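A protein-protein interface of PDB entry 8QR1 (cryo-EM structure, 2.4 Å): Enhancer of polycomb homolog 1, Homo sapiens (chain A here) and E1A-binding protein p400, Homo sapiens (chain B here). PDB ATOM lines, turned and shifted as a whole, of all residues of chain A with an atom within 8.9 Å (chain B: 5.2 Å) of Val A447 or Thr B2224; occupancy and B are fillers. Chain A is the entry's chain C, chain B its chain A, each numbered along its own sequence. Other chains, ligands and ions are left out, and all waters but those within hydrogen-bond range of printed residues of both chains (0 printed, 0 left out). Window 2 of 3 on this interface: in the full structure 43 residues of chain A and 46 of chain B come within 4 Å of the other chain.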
ATOM      1  N   THR A 444      17.350  -4.636  20.046  1.00  0.00           N
ATOM      2  CA  THR A 444      16.847  -5.388  21.185  1.00  0.00           C
ATOM      3  C   THR A 444      17.132  -4.607  22.461  1.00  0.00           C
ATOM      4  O   THR A 444      18.156  -3.926  22.568  1.00  0.00           O
ATOM      5  CB  THR A 444      17.492  -6.787  21.237  1.00  0.00           C
ATOM      6  OG1 THR A 444      17.134  -7.523  20.062  1.00  0.00           O
ATOM      7  CG2 THR A 444      17.052  -7.565  22.456  1.00  0.00           C
ATOM      8  N   LEU A 445      16.219  -4.714  23.426  1.00  0.00           N
ATOM      9  CA  LEU A 445      16.239  -3.949  24.665  1.00  0.00           C
ATOM     10  C   LEU A 445      16.505  -4.862  25.857  1.00  0.00           C
ATOM     11  O   LEU A 445      16.132  -6.038  25.860  1.00  0.00           O
ATOM     12  CB  LEU A 445      14.913  -3.208  24.851  1.00  0.00           C
ATOM     13  CG  LEU A 445      14.447  -2.333  23.682  1.00  0.00           C
ATOM     14  CD1 LEU A 445      13.089  -1.731  23.962  1.00  0.00           C
ATOM     15  CD2 LEU A 445      15.445  -1.239  23.392  1.00  0.00           C
ATOM     16  N   THR A 446      17.158  -4.303  26.885  1.00  0.00           N
ATOM     17  CA  THR A 446      17.549  -5.118  28.035  1.00  0.00           C
ATOM     18  C   THR A 446      16.349  -5.443  28.915  1.00  0.00           C
ATOM     19  O   THR A 446      16.293  -6.520  29.522  1.00  0.00           O
ATOM     20  CB  THR A 446      18.653  -4.442  28.864  1.00  0.00           C
ATOM     21  OG1 THR A 446      18.938  -5.247  30.015  1.00  0.00           O
ATOM     22  CG2 THR A 446      18.281  -3.032  29.344  1.00  0.00           C
ATOM     23  N   VAL A 447      15.395  -4.524  29.011  1.00  0.00           N
ATOM     24  CA  VAL A 447      14.099  -4.897  29.583  1.00  0.00           C
ATOM     25  C   VAL A 447      13.493  -5.947  28.660  1.00  0.00           C
ATOM     26  O   VAL A 447      13.696  -5.857  27.432  1.00  0.00           O
ATOM     27  CB  VAL A 447      13.187  -3.660  29.722  1.00  0.00           C
ATOM     28  CG1 VAL A 447      11.890  -3.979  30.453  1.00  0.00           C
ATOM     29  CG2 VAL A 447      13.915  -2.561  30.488  1.00  0.00           C
ATOM     30  N   PRO A 448      12.767  -6.966  29.148  1.00  0.00           N
ATOM     31  CA  PRO A 448      12.517  -8.152  28.300  1.00  0.00           C
ATOM     32  C   PRO A 448      11.672  -7.934  27.039  1.00  0.00           C
ATOM     33  O   PRO A 448      11.394  -8.927  26.356  1.00  0.00           O
ATOM     34  CB  PRO A 448      11.817  -9.132  29.256  1.00  0.00           C
ATOM     35  CG  PRO A 448      12.158  -8.667  30.600  1.00  0.00           C
ATOM     36  CD  PRO A 448      12.222  -7.194  30.504  1.00  0.00           C
ATOM     37  N   GLN A 449      11.288  -6.707  26.673  1.00  0.00           N
ATOM     38  CA  GLN A 449      10.541  -6.510  25.436  1.00  0.00           C
ATOM     39  C   GLN A 449      11.388  -6.622  24.170  1.00  0.00           C
ATOM     40  O   GLN A 449      11.493  -5.654  23.410  1.00  0.00           O
ATOM     41  CB  GLN A 449       9.834  -5.152  25.440  1.00  0.00           C
ATOM     42  CG  GLN A 449       8.954  -4.914  26.657  1.00  0.00           C
ATOM     43  CD  GLN A 449       9.552  -3.978  27.695  1.00  0.00           C
ATOM     44  OE1 GLN A 449      10.744  -3.671  27.678  1.00  0.00           O
ATOM     45  NE2 GLN A 449       8.709  -3.521  28.614  1.00  0.00           N
ATOM     46  N   ARG A 450      11.960  -7.805  23.929  1.00  0.00           N
ATOM     47  CA  ARG A 450      12.120  -8.450  22.623  1.00  0.00           C
ATOM     48  C   ARG A 450      12.802  -7.601  21.552  1.00  0.00           C
ATOM     49  O   ARG A 450      13.396  -6.559  21.842  1.00  0.00           O
ATOM     50  CB  ARG A 450      10.760  -8.983  22.095  1.00  0.00           C
ATOM     51  CG  ARG A 450       9.626  -8.053  21.505  1.00  0.00           C
ATOM     52  CD  ARG A 450       8.729  -7.302  22.494  1.00  0.00           C
ATOM     53  NE  ARG A 450       7.458  -6.863  21.930  1.00  0.00           N
ATOM     54  CZ  ARG A 450       6.324  -6.702  22.608  1.00  0.00           C
ATOM     55  NH1 ARG A 450       6.254  -6.880  23.921  1.00  0.00           N
ATOM     56  NH2 ARG A 450       5.230  -6.324  21.954  1.00  0.00           N
ATOM     57  N   CYS A 451      12.796  -8.104  20.318  1.00  0.00           N
ATOM     58  CA  CYS A 451      13.235  -7.331  19.166  1.00  0.00           C
ATOM     59  C   CYS A 451      12.115  -6.401  18.723  1.00  0.00           C
ATOM     60  O   CYS A 451      11.013  -6.858  18.405  1.00  0.00           O
ATOM     61  CB  CYS A 451      13.634  -8.268  18.029  1.00  0.00           C
ATOM     62  SG  CYS A 451      14.107  -7.446  16.499  1.00  0.00           S
ATOM     63  N   ILE A 452      12.404  -5.102  18.693  1.00  0.00           N
ATOM     64  CA  ILE A 452      11.416  -4.092  18.322  1.00  0.00           C
ATOM     65  C   ILE A 452      11.425  -3.824  16.819  1.00  0.00           C
ATOM     66  O   ILE A 452      10.807  -2.859  16.356  1.00  0.00           O
ATOM     67  CB  ILE A 452      11.636  -2.788  19.119  1.00  0.00           C
ATOM     68  CG1 ILE A 452      13.027  -2.170  18.885  1.00  0.00           C
ATOM     69  CG2 ILE A 452      11.440  -3.058  20.603  1.00  0.00           C
ATOM     70  CD1 ILE A 452      13.180  -0.793  19.460  1.00  0.00           C
ATOM     71  N   ARG A 457      18.533   5.421  16.518  1.00  0.00           N
ATOM     72  CA  ARG A 457      18.649   6.234  17.719  1.00  0.00           C
ATOM     73  C   ARG A 457      18.770   7.693  17.308  1.00  0.00           C
ATOM     74  O   ARG A 457      19.604   8.035  16.464  1.00  0.00           O
ATOM     75  CB  ARG A 457      19.861   5.814  18.542  1.00  0.00           C
ATOM     76  CG  ARG A 457      19.763   4.425  19.118  1.00  0.00           C
ATOM     77  CD  ARG A 457      20.987   4.088  19.934  1.00  0.00           C
ATOM     78  NE  ARG A 457      20.921   4.692  21.261  1.00  0.00           N
ATOM     79  CZ  ARG A 457      21.950   5.132  21.978  1.00  0.00           C
ATOM     80  NH1 ARG A 457      23.198   5.063  21.539  1.00  0.00           N
ATOM     81  NH2 ARG A 457      21.721   5.653  23.178  1.00  0.00           N
ATOM     82  N   ARG A 464      16.852  14.344  25.157  1.00  0.00           N
ATOM     83  CA  ARG A 464      16.269  13.029  25.362  1.00  0.00           C
ATOM     84  C   ARG A 464      16.522  12.147  24.150  1.00  0.00           C
ATOM     85  O   ARG A 464      16.252  12.541  23.012  1.00  0.00           O
ATOM     86  CB  ARG A 464      14.767  13.152  25.618  1.00  0.00           C
ATOM     87  CG  ARG A 464      14.400  14.089  26.762  1.00  0.00           C
ATOM     88  CD  ARG A 464      12.911  14.231  26.939  1.00  0.00           C
ATOM     89  NE  ARG A 464      12.370  13.200  27.824  1.00  0.00           N
ATOM     90  CZ  ARG A 464      11.474  12.266  27.517  1.00  0.00           C
ATOM     91  NH1 ARG A 464      10.922  12.175  26.317  1.00  0.00           N
ATOM     92  NH2 ARG A 464      11.112  11.396  28.451  1.00  0.00           N
ATOM     93  N   VAL A 465      17.035  10.947  24.403  1.00  0.00           N
ATOM     94  CA  VAL A 465      17.398   9.998  23.359  1.00  0.00           C
ATOM     95  C   VAL A 465      16.213   9.082  23.109  1.00  0.00           C
ATOM     96  O   VAL A 465      15.764   8.374  24.018  1.00  0.00           O
ATOM     97  CB  VAL A 465      18.643   9.186  23.751  1.00  0.00           C
ATOM     98  CG1 VAL A 465      19.004   8.213  22.635  1.00  0.00           C
ATOM     99  CG2 VAL A 465      19.800  10.121  24.086  1.00  0.00           C
ATOM    100  N   LEU A 466      15.716   9.092  21.875  1.00  0.00           N
ATOM    101  CA  LEU A 466      14.548   8.330  21.464  1.00  0.00           C
ATOM    102  C   LEU A 466      14.960   7.230  20.501  1.00  0.00           C
ATOM    103  O   LEU A 466      16.080   7.226  19.980  1.00  0.00           O
ATOM    104  CB  LEU A 466      13.511   9.219  20.785  1.00  0.00           C
ATOM    105  CG  LEU A 466      13.313  10.645  21.299  1.00  0.00           C
ATOM    106  CD1 LEU A 466      12.222  11.318  20.521  1.00  0.00           C
ATOM    107  CD2 LEU A 466      12.970  10.666  22.763  1.00  0.00           C
ATOM    108  N   LEU A 467      14.037   6.297  20.280  1.00  0.00           N
ATOM    109  CA  LEU A 467      14.193   5.219  19.310  1.00  0.00           C
ATOM    110  C   LEU A 467      13.083   5.334  18.276  1.00  0.00           C
ATOM    111  O   LEU A 467      11.918   5.061  18.574  1.00  0.00           O
ATOM    112  CB  LEU A 467      14.141   3.853  19.988  1.00  0.00           C
ATOM    113  CG  LEU A 467      15.426   3.269  20.573  1.00  0.00           C
ATOM    114  CD1 LEU A 467      15.098   2.059  21.411  1.00  0.00           C
ATOM    115  CD2 LEU A 467      16.410   2.897  19.488  1.00  0.00           C
ATOM    116  N   THR B2222       7.130   3.267  24.925  1.00  0.00           N
ATOM    117  CA  THR B2222       8.054   3.774  25.923  1.00  0.00           C
ATOM    118  C   THR B2222       9.099   2.705  26.209  1.00  0.00           C
ATOM    119  O   THR B2222       8.832   1.505  26.114  1.00  0.00           O
ATOM    120  CB  THR B2222       7.285   4.175  27.191  1.00  0.00           C
ATOM    121  OG1 THR B2222       6.436   5.291  26.903  1.00  0.00           O
ATOM    122  CG2 THR B2222       8.191   4.574  28.308  1.00  0.00           C
ATOM    123  N   TYR B2223      10.299   3.165  26.549  1.00  0.00           N
ATOM    124  CA  TYR B2223      11.400   2.305  26.946  1.00  0.00           C
ATOM    125  C   TYR B2223      12.182   3.017  28.038  1.00  0.00           C
ATOM    126  O   TYR B2223      12.080   4.233  28.206  1.00  0.00           O
ATOM    127  CB  TYR B2223      12.268   1.926  25.738  1.00  0.00           C
ATOM    128  CG  TYR B2223      13.244   2.969  25.253  1.00  0.00           C
ATOM    129  CD1 TYR B2223      12.837   4.261  24.969  1.00  0.00           C
ATOM    130  CD2 TYR B2223      14.564   2.639  25.015  1.00  0.00           C
ATOM    131  CE1 TYR B2223      13.724   5.201  24.510  1.00  0.00           C
ATOM    132  CE2 TYR B2223      15.457   3.571  24.552  1.00  0.00           C
ATOM    133  CZ  TYR B2223      15.031   4.850  24.297  1.00  0.00           C
ATOM    134  OH  TYR B2223      15.922   5.784  23.834  1.00  0.00           O
ATOM    135  N   THR B2224      12.939   2.245  28.806  1.00  0.00           N
ATOM    136  CA  THR B2224      13.453   2.736  30.074  1.00  0.00           C
ATOM    137  C   THR B2224      14.671   3.634  29.883  1.00  0.00           C
ATOM    138  O   THR B2224      15.262   3.704  28.802  1.00  0.00           O
ATOM    139  CB  THR B2224      13.791   1.564  30.999  1.00  0.00           C
ATOM    140  OG1 THR B2224      13.933   2.032  32.346  1.00  0.00           O
ATOM    141  CG2 THR B2224      15.062   0.863  30.569  1.00  0.00           C
ATOM    142  N   ARG B2225      15.030   4.330  30.963  1.00  0.00           N
ATOM    143  CA  ARG B2225      16.163   5.250  30.949  1.00  0.00           C
ATOM    144  C   ARG B2225      17.469   4.525  30.659  1.00  0.00           C
ATOM    145  O   ARG B2225      18.321   5.031  29.917  1.00  0.00           O
ATOM    146  CB  ARG B2225      16.230   5.973  32.297  1.00  0.00           C
ATOM    147  CG  ARG B2225      17.390   6.932  32.498  1.00  0.00           C
ATOM    148  CD  ARG B2225      17.312   7.601  33.849  1.00  0.00           C
ATOM    149  NE  ARG B2225      16.259   8.606  33.907  1.00  0.00           N
ATOM    150  CZ  ARG B2225      16.350   9.839  33.423  1.00  0.00           C
ATOM    151  NH1 ARG B2225      17.437  10.272  32.802  1.00  0.00           N
ATOM    152  NH2 ARG B2225      15.322  10.665  33.566  1.00  0.00           N
ATOM    153  N   GLU B2226      17.651   3.348  31.259  1.00  0.00           N
ATOM    154  CA  GLU B2226      18.903   2.616  31.113  1.00  0.00           C
ATOM    155  C   GLU B2226      19.145   2.202  29.671  1.00  0.00           C
ATOM    156  O   GLU B2226      20.277   2.288  29.188  1.00  0.00           O
ATOM    157  CB  GLU B2226      18.902   1.393  32.028  1.00  0.00           C
ATOM    158  CG  GLU B2226      19.002   1.720  33.525  1.00  0.00           C
ATOM    159  CD  GLU B2226      17.680   2.119  34.171  1.00  0.00           C
ATOM    160  OE1 GLU B2226      16.614   1.973  33.538  1.00  0.00           O
ATOM    161  OE2 GLU B2226      17.712   2.590  35.328  1.00  0.00           O
ATOM    162  N   ASP B2227      18.101   1.765  28.969  1.00  0.00           N
ATOM    163  CA  ASP B2227      18.222   1.487  27.543  1.00  0.00           C
ATOM    164  C   ASP B2227      18.558   2.746  26.759  1.00  0.00           C
ATOM    165  O   ASP B2227      19.384   2.705  25.841  1.00  0.00           O
ATOM    166  CB  ASP B2227      16.920   0.892  27.004  1.00  0.00           C
ATOM    167  CG  ASP B2227      16.928  -0.616  26.971  1.00  0.00           C
ATOM    168  OD1 ASP B2227      17.886  -1.203  26.427  1.00  0.00           O
ATOM    169  OD2 ASP B2227      15.974  -1.221  27.500  1.00  0.00           O
ATOM    170  N   ALA B2228      17.912   3.862  27.096  1.00  0.00           N
ATOM    171  CA  ALA B2228      18.059   5.082  26.311  1.00  0.00           C
ATOM    172  C   ALA B2228      19.474   5.631  26.399  1.00  0.00           C
ATOM    173  O   ALA B2228      20.063   6.022  25.384  1.00  0.00           O
ATOM    174  CB  ALA B2228      17.052   6.124  26.784  1.00  0.00           C
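The side-chain carboxylate (OD1) of Asp B2227 is in hydrogen-bond range of the backbone NH (N) of Thr A446 (3.2 Å). The side-chain hydroxyl (OH) of Tyr B2223 sits at hydrogen-bond distance from the backbone carbonyl oxygen (O) of Val A465 (2.6 Å). NH2 of Arg A457 is in hydrogen-bond range of O of Ala B2228, 2.8 Å away.
The side-chain hydroxyl of Thr B2224 sits at hydrogen-bond distance from the side-chain carboxylate of Glu B2226, 2.9 Å away.
Leu A445 touches Asp B2227 (CB to OD2, 3.5 Å). CG2 of Thr B2224 touches CG2 of Val A447, at 3.6 Å. N of Val A447 touches OD2 of Asp B2227, at 3.7 Å. Ala B2228 touches Val A465 (O to CG1, 3.7 Å). CA of Leu A466 touches OH of Tyr B2223, 3.7 Å away. Leu A467 touches Tyr B2223 (CD1 to CE2, 3.5 Å).
Gln A449 touches none of the printed residues of chain B. Cys A451 touches none of the printed residues of chain B. Printed residues of chain B within 4 Å of Leu A467: Tyr B2223. Of the printed residues of chain A, Thr B2224 touches Val A447 (3.6 Å). Printed residues of chain A within 4 Å of Asp B2227: Leu A445, Thr A446 and Val A447. The nearest printed residue of chain B that does not touch Val A447 is Glu B2226 (6.1 Å). The nearest residue of chain A that does not touch Thr B2224 is Thr A446 (5.2 Å).
Of the 14 printed residues of chain A, 7 touch a printed residue of chain B. Hydrophobic or aromatic side chains of chain A within 4 Å of the printed part of chain B: Leu A445, Val A447, Val A465 and Leu A467. Of the 7 printed residues of chain B, 4 touch a printed residue of chain A. Among the printed residues, no Asp or Glu carboxylate lies within 4 Å of a Lys or Arg side-chain nitrogen of the other chain.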
